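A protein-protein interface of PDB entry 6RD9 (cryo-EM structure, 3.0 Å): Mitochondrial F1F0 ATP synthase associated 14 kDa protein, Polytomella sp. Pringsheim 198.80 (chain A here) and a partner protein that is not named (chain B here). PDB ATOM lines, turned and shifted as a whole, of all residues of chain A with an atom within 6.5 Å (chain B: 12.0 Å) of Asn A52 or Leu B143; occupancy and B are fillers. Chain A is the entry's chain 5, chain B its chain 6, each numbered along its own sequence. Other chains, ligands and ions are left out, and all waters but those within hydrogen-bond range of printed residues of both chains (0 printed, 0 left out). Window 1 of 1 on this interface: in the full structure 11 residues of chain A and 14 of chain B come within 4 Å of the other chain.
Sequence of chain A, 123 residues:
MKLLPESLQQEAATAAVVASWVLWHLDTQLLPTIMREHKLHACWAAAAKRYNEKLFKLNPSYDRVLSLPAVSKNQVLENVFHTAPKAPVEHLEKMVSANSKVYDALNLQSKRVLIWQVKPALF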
ATOM      1  N   TRP A  44     -10.508 -24.025  22.042  1.00  0.00           N
ATOM      2  CA  TRP A  44      -9.160 -24.077  21.521  1.00  0.00           C
ATOM      3  C   TRP A  44      -8.993 -23.162  20.331  1.00  0.00           C
ATOM      4  O   TRP A  44      -7.900 -22.681  20.075  1.00  0.00           O
ATOM      5  CB  TRP A  44      -8.809 -25.496  21.133  1.00  0.00           C
ATOM      6  CG  TRP A  44      -8.104 -26.266  22.161  1.00  0.00           C
ATOM      7  CD1 TRP A  44      -8.524 -27.399  22.736  1.00  0.00           C
ATOM      8  CD2 TRP A  44      -6.829 -25.982  22.720  1.00  0.00           C
ATOM      9  NE1 TRP A  44      -7.605 -27.853  23.625  1.00  0.00           N
ATOM     10  CE2 TRP A  44      -6.551 -26.987  23.634  1.00  0.00           C
ATOM     11  CE3 TRP A  44      -5.907 -24.953  22.558  1.00  0.00           C
ATOM     12  CZ2 TRP A  44      -5.393 -27.004  24.366  1.00  0.00           C
ATOM     13  CZ3 TRP A  44      -4.777 -24.988  23.248  1.00  0.00           C
ATOM     14  CH2 TRP A  44      -4.517 -25.996  24.154  1.00  0.00           C
ATOM     15  N   ALA A  47      -9.059 -19.497  21.997  1.00  0.00           N
ATOM     16  CA  ALA A  47      -7.931 -19.162  22.835  1.00  0.00           C
ATOM     17  C   ALA A  47      -6.609 -19.245  22.132  1.00  0.00           C
ATOM     18  O   ALA A  47      -5.647 -18.723  22.679  1.00  0.00           O
ATOM     19  CB  ALA A  47      -7.838 -20.081  24.029  1.00  0.00           C
ATOM     20  N   ALA A  48      -6.546 -19.845  20.938  1.00  0.00           N
ATOM     21  CA  ALA A  48      -5.289 -20.247  20.309  1.00  0.00           C
ATOM     22  C   ALA A  48      -4.325 -19.105  20.115  1.00  0.00           C
ATOM     23  O   ALA A  48      -3.113 -19.307  20.149  1.00  0.00           O
ATOM     24  CB  ALA A  48      -5.545 -20.848  18.946  1.00  0.00           C
ATOM     25  N   LYS A  49      -4.832 -17.908  19.895  1.00  0.00           N
ATOM     26  CA  LYS A  49      -3.959 -16.773  19.690  1.00  0.00           C
ATOM     27  C   LYS A  49      -3.459 -16.221  21.007  1.00  0.00           C
ATOM     28  O   LYS A  49      -2.310 -15.797  21.101  1.00  0.00           O
ATOM     29  CB  LYS A  49      -4.694 -15.707  18.907  1.00  0.00           C
ATOM     30  CG  LYS A  49      -3.801 -14.694  18.306  1.00  0.00           C
ATOM     31  CD  LYS A  49      -4.571 -13.471  17.917  1.00  0.00           C
ATOM     32  CE  LYS A  49      -3.621 -12.365  17.543  1.00  0.00           C
ATOM     33  NZ  LYS A  49      -2.570 -12.228  18.583  1.00  0.00           N
ATOM     34  N   ARG A  50      -4.302 -16.209  22.024  1.00  0.00           N
ATOM     35  CA  ARG A  50      -3.921 -15.718  23.334  1.00  0.00           C
ATOM     36  C   ARG A  50      -3.302 -16.784  24.202  1.00  0.00           C
ATOM     37  O   ARG A  50      -2.651 -16.449  25.182  1.00  0.00           O
ATOM     38  CB  ARG A  50      -5.134 -15.155  24.051  1.00  0.00           C
ATOM     39  CG  ARG A  50      -5.653 -13.922  23.417  1.00  0.00           C
ATOM     40  CD  ARG A  50      -6.939 -13.487  24.027  1.00  0.00           C
ATOM     41  NE  ARG A  50      -6.939 -13.604  25.472  1.00  0.00           N
ATOM     42  CZ  ARG A  50      -7.696 -12.855  26.257  1.00  0.00           C
ATOM     43  NH1 ARG A  50      -7.657 -13.020  27.569  1.00  0.00           N
ATOM     44  NH2 ARG A  50      -8.493 -11.938  25.724  1.00  0.00           N
ATOM     45  N   TYR A  51      -3.546 -18.053  23.909  1.00  0.00           N
ATOM     46  CA  TYR A  51      -2.891 -19.132  24.629  1.00  0.00           C
ATOM     47  C   TYR A  51      -1.435 -19.200  24.246  1.00  0.00           C
ATOM     48  O   TYR A  51      -0.560 -19.324  25.099  1.00  0.00           O
ATOM     49  CB  TYR A  51      -3.575 -20.443  24.292  1.00  0.00           C
ATOM     50  CG  TYR A  51      -3.163 -21.630  25.055  1.00  0.00           C
ATOM     51  CD1 TYR A  51      -3.782 -21.940  26.234  1.00  0.00           C
ATOM     52  CD2 TYR A  51      -2.203 -22.477  24.570  1.00  0.00           C
ATOM     53  CE1 TYR A  51      -3.425 -23.025  26.926  1.00  0.00           C
ATOM     54  CE2 TYR A  51      -1.843 -23.560  25.255  1.00  0.00           C
ATOM     55  CZ  TYR A  51      -2.452 -23.833  26.428  1.00  0.00           C
ATOM     56  OH  TYR A  51      -2.077 -24.943  27.107  1.00  0.00           O
ATOM     57  N   ASN A  52      -1.163 -19.131  22.956  1.00  0.00           N
ATOM     58  CA  ASN A  52       0.184 -19.265  22.454  1.00  0.00           C
ATOM     59  C   ASN A  52       1.012 -18.045  22.746  1.00  0.00           C
ATOM     60  O   ASN A  52       2.218 -18.155  22.912  1.00  0.00           O
ATOM     61  CB  ASN A  52       0.143 -19.498  20.966  1.00  0.00           C
ATOM     62  CG  ASN A  52      -0.355 -20.830  20.629  1.00  0.00           C
ATOM     63  OD1 ASN A  52      -0.015 -21.786  21.276  1.00  0.00           O
ATOM     64  ND2 ASN A  52      -1.177 -20.913  19.619  1.00  0.00           N
ATOM     65  N   GLU A  53       0.398 -16.879  22.795  1.00  0.00           N
ATOM     66  CA  GLU A  53       1.131 -15.683  23.163  1.00  0.00           C
ATOM     67  C   GLU A  53       1.394 -15.645  24.653  1.00  0.00           C
ATOM     68  O   GLU A  53       2.428 -15.145  25.080  1.00  0.00           O
ATOM     69  CB  GLU A  53       0.363 -14.455  22.712  1.00  0.00           C
ATOM     70  CG  GLU A  53       1.070 -13.144  22.926  1.00  0.00           C
ATOM     71  CD  GLU A  53       2.394 -13.042  22.202  1.00  0.00           C
ATOM     72  OE1 GLU A  53       2.406 -13.116  20.960  1.00  0.00           O
ATOM     73  OE2 GLU A  53       3.427 -12.878  22.878  1.00  0.00           O
ATOM     74  N   LYS A  54       0.494 -16.180  25.462  1.00  0.00           N
ATOM     75  CA  LYS A  54       0.758 -16.263  26.890  1.00  0.00           C
ATOM     76  C   LYS A  54       1.820 -17.294  27.196  1.00  0.00           C
ATOM     77  O   LYS A  54       2.592 -17.133  28.136  1.00  0.00           O
ATOM     78  CB  LYS A  54      -0.519 -16.596  27.641  1.00  0.00           C
ATOM     79  CG  LYS A  54      -0.410 -16.493  29.117  1.00  0.00           C
ATOM     80  CD  LYS A  54      -1.697 -16.823  29.768  1.00  0.00           C
ATOM     81  CE  LYS A  54      -1.584 -16.655  31.249  1.00  0.00           C
ATOM     82  NZ  LYS A  54      -2.812 -17.063  31.958  1.00  0.00           N
ATOM     83  N   LEU A  55       1.876 -18.349  26.415  1.00  0.00           N
ATOM     84  CA  LEU A  55       2.870 -19.384  26.603  1.00  0.00           C
ATOM     85  C   LEU A  55       4.219 -18.960  26.067  1.00  0.00           C
ATOM     86  O   LEU A  55       5.242 -19.364  26.609  1.00  0.00           O
ATOM     87  CB  LEU A  55       2.381 -20.649  25.914  1.00  0.00           C
ATOM     88  CG  LEU A  55       3.014 -21.985  26.190  1.00  0.00           C
ATOM     89  CD1 LEU A  55       3.120 -22.174  27.620  1.00  0.00           C
ATOM     90  CD2 LEU A  55       2.114 -22.983  25.640  1.00  0.00           C
ATOM     91  N   PHE A  56       4.234 -18.162  25.006  1.00  0.00           N
ATOM     92  CA  PHE A  56       5.464 -17.583  24.489  1.00  0.00           C
ATOM     93  C   PHE A  56       6.101 -16.665  25.504  1.00  0.00           C
ATOM     94  O   PHE A  56       7.319 -16.673  25.678  1.00  0.00           O
ATOM     95  CB  PHE A  56       5.152 -16.803  23.231  1.00  0.00           C
ATOM     96  CG  PHE A  56       6.335 -16.426  22.437  1.00  0.00           C
ATOM     97  CD1 PHE A  56       7.003 -17.366  21.711  1.00  0.00           C
ATOM     98  CD2 PHE A  56       6.750 -15.123  22.372  1.00  0.00           C
ATOM     99  CE1 PHE A  56       8.076 -17.019  20.966  1.00  0.00           C
ATOM    100  CE2 PHE A  56       7.826 -14.784  21.623  1.00  0.00           C
ATOM    101  CZ  PHE A  56       8.482 -15.731  20.919  1.00  0.00           C
ATOM    102  N   LYS A  57       5.294 -15.884  26.208  1.00  0.00           N
ATOM    103  CA  LYS A  57       5.832 -14.993  27.215  1.00  0.00           C
ATOM    104  C   LYS A  57       6.264 -15.722  28.465  1.00  0.00           C
ATOM    105  O   LYS A  57       6.958 -15.136  29.291  1.00  0.00           O
ATOM    106  CB  LYS A  57       4.803 -13.947  27.588  1.00  0.00           C
ATOM    107  CG  LYS A  57       4.455 -13.006  26.483  1.00  0.00           C
ATOM    108  CD  LYS A  57       3.306 -12.127  26.907  1.00  0.00           C
ATOM    109  CE  LYS A  57       2.724 -11.392  25.729  1.00  0.00           C
ATOM    110  NZ  LYS A  57       1.421 -10.752  26.031  1.00  0.00           N
ATOM    111  N   VAL B  32       4.842 -38.512  30.606  1.00  0.00           N
ATOM    112  CA  VAL B  32       6.016 -37.683  30.408  1.00  0.00           C
ATOM    113  C   VAL B  32       6.923 -37.762  31.621  1.00  0.00           C
ATOM    114  O   VAL B  32       8.140 -37.857  31.482  1.00  0.00           O
ATOM    115  CB  VAL B  32       5.583 -36.253  30.080  1.00  0.00           C
ATOM    116  CG1 VAL B  32       6.752 -35.383  29.943  1.00  0.00           C
ATOM    117  CG2 VAL B  32       4.872 -36.270  28.794  1.00  0.00           C
ATOM    118  N   THR B 139      -9.801 -28.191  11.627  1.00  0.00           N
ATOM    119  CA  THR B 139      -8.830 -28.900  12.435  1.00  0.00           C
ATOM    120  C   THR B 139      -8.713 -28.147  13.751  1.00  0.00           C
ATOM    121  O   THR B 139      -9.052 -26.967  13.815  1.00  0.00           O
ATOM    122  CB  THR B 139      -7.486 -28.942  11.712  1.00  0.00           C
ATOM    123  OG1 THR B 139      -7.719 -29.235  10.337  1.00  0.00           O
ATOM    124  CG2 THR B 139      -6.593 -30.051  12.247  1.00  0.00           C
ATOM    125  N   LEU B 140      -8.262 -28.823  14.805  1.00  0.00           N
ATOM    126  CA  LEU B 140      -7.968 -28.124  16.044  1.00  0.00           C
ATOM    127  C   LEU B 140      -6.854 -27.112  15.862  1.00  0.00           C
ATOM    128  O   LEU B 140      -5.972 -27.270  15.025  1.00  0.00           O
ATOM    129  CB  LEU B 140      -7.571 -29.084  17.139  1.00  0.00           C
ATOM    130  CG  LEU B 140      -8.686 -29.581  18.002  1.00  0.00           C
ATOM    131  CD1 LEU B 140      -8.029 -30.400  18.975  1.00  0.00           C
ATOM    132  CD2 LEU B 140      -9.282 -28.424  18.683  1.00  0.00           C
ATOM    133  N   ASN B 141      -6.881 -26.075  16.682  1.00  0.00           N
ATOM    134  CA  ASN B 141      -6.153 -24.881  16.344  1.00  0.00           C
ATOM    135  C   ASN B 141      -5.165 -24.379  17.378  1.00  0.00           C
ATOM    136  O   ASN B 141      -4.352 -23.523  17.034  1.00  0.00           O
ATOM    137  CB  ASN B 141      -7.121 -23.747  16.036  1.00  0.00           C
ATOM    138  CG  ASN B 141      -6.565 -22.785  15.045  1.00  0.00           C
ATOM    139  OD1 ASN B 141      -5.699 -23.140  14.255  1.00  0.00           O
ATOM    140  ND2 ASN B 141      -7.042 -21.550  15.084  1.00  0.00           N
ATOM    141  N   GLY B 142      -5.177 -24.845  18.606  1.00  0.00           N
ATOM    142  CA  GLY B 142      -4.261 -24.282  19.574  1.00  0.00           C
ATOM    143  C   GLY B 142      -2.856 -24.813  19.455  1.00  0.00           C
ATOM    144  O   GLY B 142      -2.529 -25.552  18.536  1.00  0.00           O
ATOM    145  N   LEU B 143      -2.004 -24.350  20.369  1.00  0.00           N
ATOM    146  CA  LEU B 143      -0.713 -24.939  20.746  1.00  0.00           C
ATOM    147  C   LEU B 143       0.217 -25.161  19.551  1.00  0.00           C
ATOM    148  O   LEU B 143       0.299 -26.243  18.988  1.00  0.00           O
ATOM    149  CB  LEU B 143      -0.877 -26.211  21.554  1.00  0.00           C
ATOM    150  CG  LEU B 143       0.440 -26.405  22.293  1.00  0.00           C
ATOM    151  CD1 LEU B 143       0.555 -25.436  23.368  1.00  0.00           C
ATOM    152  CD2 LEU B 143       0.567 -27.729  22.869  1.00  0.00           C
ATOM    153  N   LYS B 144       0.832 -24.067  19.105  1.00  0.00           N
ATOM    154  CA  LYS B 144       1.553 -24.038  17.844  1.00  0.00           C
ATOM    155  C   LYS B 144       3.039 -24.331  17.959  1.00  0.00           C
ATOM    156  O   LYS B 144       3.820 -23.716  17.219  1.00  0.00           O
ATOM    157  CB  LYS B 144       1.333 -22.706  17.137  1.00  0.00           C
ATOM    158  CG  LYS B 144      -0.039 -22.552  16.635  1.00  0.00           C
ATOM    159  CD  LYS B 144      -0.271 -23.571  15.580  1.00  0.00           C
ATOM    160  CE  LYS B 144      -1.702 -23.576  15.146  1.00  0.00           C
ATOM    161  NZ  LYS B 144      -1.987 -24.695  14.217  1.00  0.00           N
ATOM    162  N   THR B 145       3.467 -25.176  18.899  1.00  0.00           N
ATOM    163  CA  THR B 145       4.746 -25.906  18.882  1.00  0.00           C
ATOM    164  C   THR B 145       5.995 -25.050  19.088  1.00  0.00           C
ATOM    165  O   THR B 145       6.891 -25.455  19.827  1.00  0.00           O
ATOM    166  CB  THR B 145       4.893 -26.683  17.557  1.00  0.00           C
ATOM    167  OG1 THR B 145       3.919 -27.727  17.492  1.00  0.00           O
ATOM    168  CG2 THR B 145       6.256 -27.327  17.403  1.00  0.00           C
ATOM    169  N   PHE B 146       6.002 -23.809  18.625  1.00  0.00           N
ATOM    170  CA  PHE B 146       7.085 -22.893  18.925  1.00  0.00           C
ATOM    171  C   PHE B 146       6.891 -22.193  20.240  1.00  0.00           C
ATOM    172  O   PHE B 146       7.832 -21.575  20.736  1.00  0.00           O
ATOM    173  CB  PHE B 146       7.217 -21.836  17.836  1.00  0.00           C
ATOM    174  CG  PHE B 146       8.388 -22.022  16.936  1.00  0.00           C
ATOM    175  CD1 PHE B 146       9.551 -21.341  17.179  1.00  0.00           C
ATOM    176  CD2 PHE B 146       8.339 -22.878  15.867  1.00  0.00           C
ATOM    177  CE1 PHE B 146      10.627 -21.486  16.353  1.00  0.00           C
ATOM    178  CE2 PHE B 146       9.417 -23.030  15.052  1.00  0.00           C
ATOM    179  CZ  PHE B 146      10.558 -22.338  15.294  1.00  0.00           C
ATOM    180  N   SER B 147       5.696 -22.256  20.797  1.00  0.00           N
ATOM    181  CA  SER B 147       5.454 -21.661  22.088  1.00  0.00           C
ATOM    182  C   SER B 147       5.743 -22.617  23.220  1.00  0.00           C
ATOM    183  O   SER B 147       6.016 -22.174  24.330  1.00  0.00           O
ATOM    184  CB  SER B 147       4.021 -21.172  22.169  1.00  0.00           C
ATOM    185  OG  SER B 147       3.141 -22.248  22.012  1.00  0.00           O
ATOM    186  N   SER B 148       5.723 -23.915  22.964  1.00  0.00           N
ATOM    187  CA  SER B 148       5.849 -24.903  24.021  1.00  0.00           C
ATOM    188  C   SER B 148       7.127 -25.713  23.915  1.00  0.00           C
ATOM    189  O   SER B 148       7.141 -26.870  24.329  1.00  0.00           O
ATOM    190  CB  SER B 148       4.651 -25.835  24.003  1.00  0.00           C
ATOM    191  OG  SER B 148       4.506 -26.382  22.715  1.00  0.00           O
ATOM    192  N   ILE B 149       8.199 -25.152  23.373  1.00  0.00           N
ATOM    193  CA  ILE B 149       9.455 -25.877  23.349  1.00  0.00           C
ATOM    194  C   ILE B 149      10.088 -25.838  24.730  1.00  0.00           C
ATOM    195  O   ILE B 149       9.753 -25.013  25.574  1.00  0.00           O
ATOM    196  CB  ILE B 149      10.421 -25.304  22.318  1.00  0.00           C
ATOM    197  CG1 ILE B 149      10.622 -23.870  22.666  1.00  0.00           C
ATOM    198  CG2 ILE B 149       9.922 -25.418  20.932  1.00  0.00           C
ATOM    199  CD1 ILE B 149      11.833 -23.408  22.185  1.00  0.00           C
ATOM    200  N   SER B 150      11.033 -26.742  24.956  1.00  0.00           N
ATOM    201  CA  SER B 150      11.810 -26.756  26.192  1.00  0.00           C
ATOM    202  C   SER B 150      13.272 -26.951  25.797  1.00  0.00           C
ATOM    203  O   SER B 150      13.774 -28.072  25.757  1.00  0.00           O
ATOM    204  CB  SER B 150      11.333 -27.850  27.126  1.00  0.00           C
ATOM    205  OG  SER B 150       9.979 -27.703  27.458  1.00  0.00           O
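The side-chain amide oxygen (OD1) of Asn A52 sits at hydrogen-bond distance from the side-chain hydroxyl (OG) of Ser B147 (3.3 Å). The backbone NH (N) of Leu B143 lies close to the side-chain amide oxygen (OD1) of Asn A52. N of Lys B144 is in hydrogen-bond range of OD1 of Asn A52, at 3.3 Å.
Tyr A51 touches just one residue of chain B: Leu B143. Of chain B, only Leu B143 (3.3 Å), Lys B144 (3.3 Å) and Ser B147 (3.3 Å) come within 4 Å of Asn A52. No residue of chain B comes within 4 Å of Glu A53. Phe A56 touches none of the printed residues of chain B. Printed residues of chain A within 4 Å of Leu B140: Trp A44 (3.8 Å). Printed residues of chain A within 4 Å of Gly B142: Trp A44 (3.5 Å) and Ala A48 (3.7 Å). Leu B143 touches just these residues of chain A: Tyr A51 (3.6 Å), Asn A52 (3.3 Å) and Leu A55 (3.7 Å). Printed residues of chain A within 4 Å of Ser B147: Asn A52 and Leu A55. The nearest residue of chain A that does not touch Leu B143 is Trp A44 (4.05 Å).
Among the printed residues, merely in contact across the chains: Trp A44 with Leu B140 (3.8 Å), Trp A44 with Gly B142 (3.5 Å), Ala A48 with Asn B141 (3.5 Å), Ala A48 with Gly B142 (3.7 Å), Tyr A51 with Leu B143 (3.6 Å), Leu A55 with Leu B143 (3.7 Å) and Leu A55 with Ser B147 (3.5 Å).
The backbone carbonyl oxygen (O) of Ala A48 sits at hydrogen-bond distance from the side-chain amide nitrogen (ND2) of Asn A52 (2.6 Å).
Of the 12 printed residues of chain A, 5 touch a printed residue of chain B. Hydrophobic or aromatic side chains of chain A within 4 Å of the printed part of chain B: Trp A44, Ala A48, Tyr A51 and Leu A55. Printed residues of chain B that touch a printed residue of chain A: Leu B140, Asn B141, Gly B142, Leu B143, Lys B144 and Ser B147. Hydrophobic or aromatic side chains of chain B that line the printed part of chain A: Leu B140 and Leu B143. Along chain B the printed residues that touch a printed residue of chain A span positions 140 to 147. Among the printed residues, 10 pairs touch across the chains.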
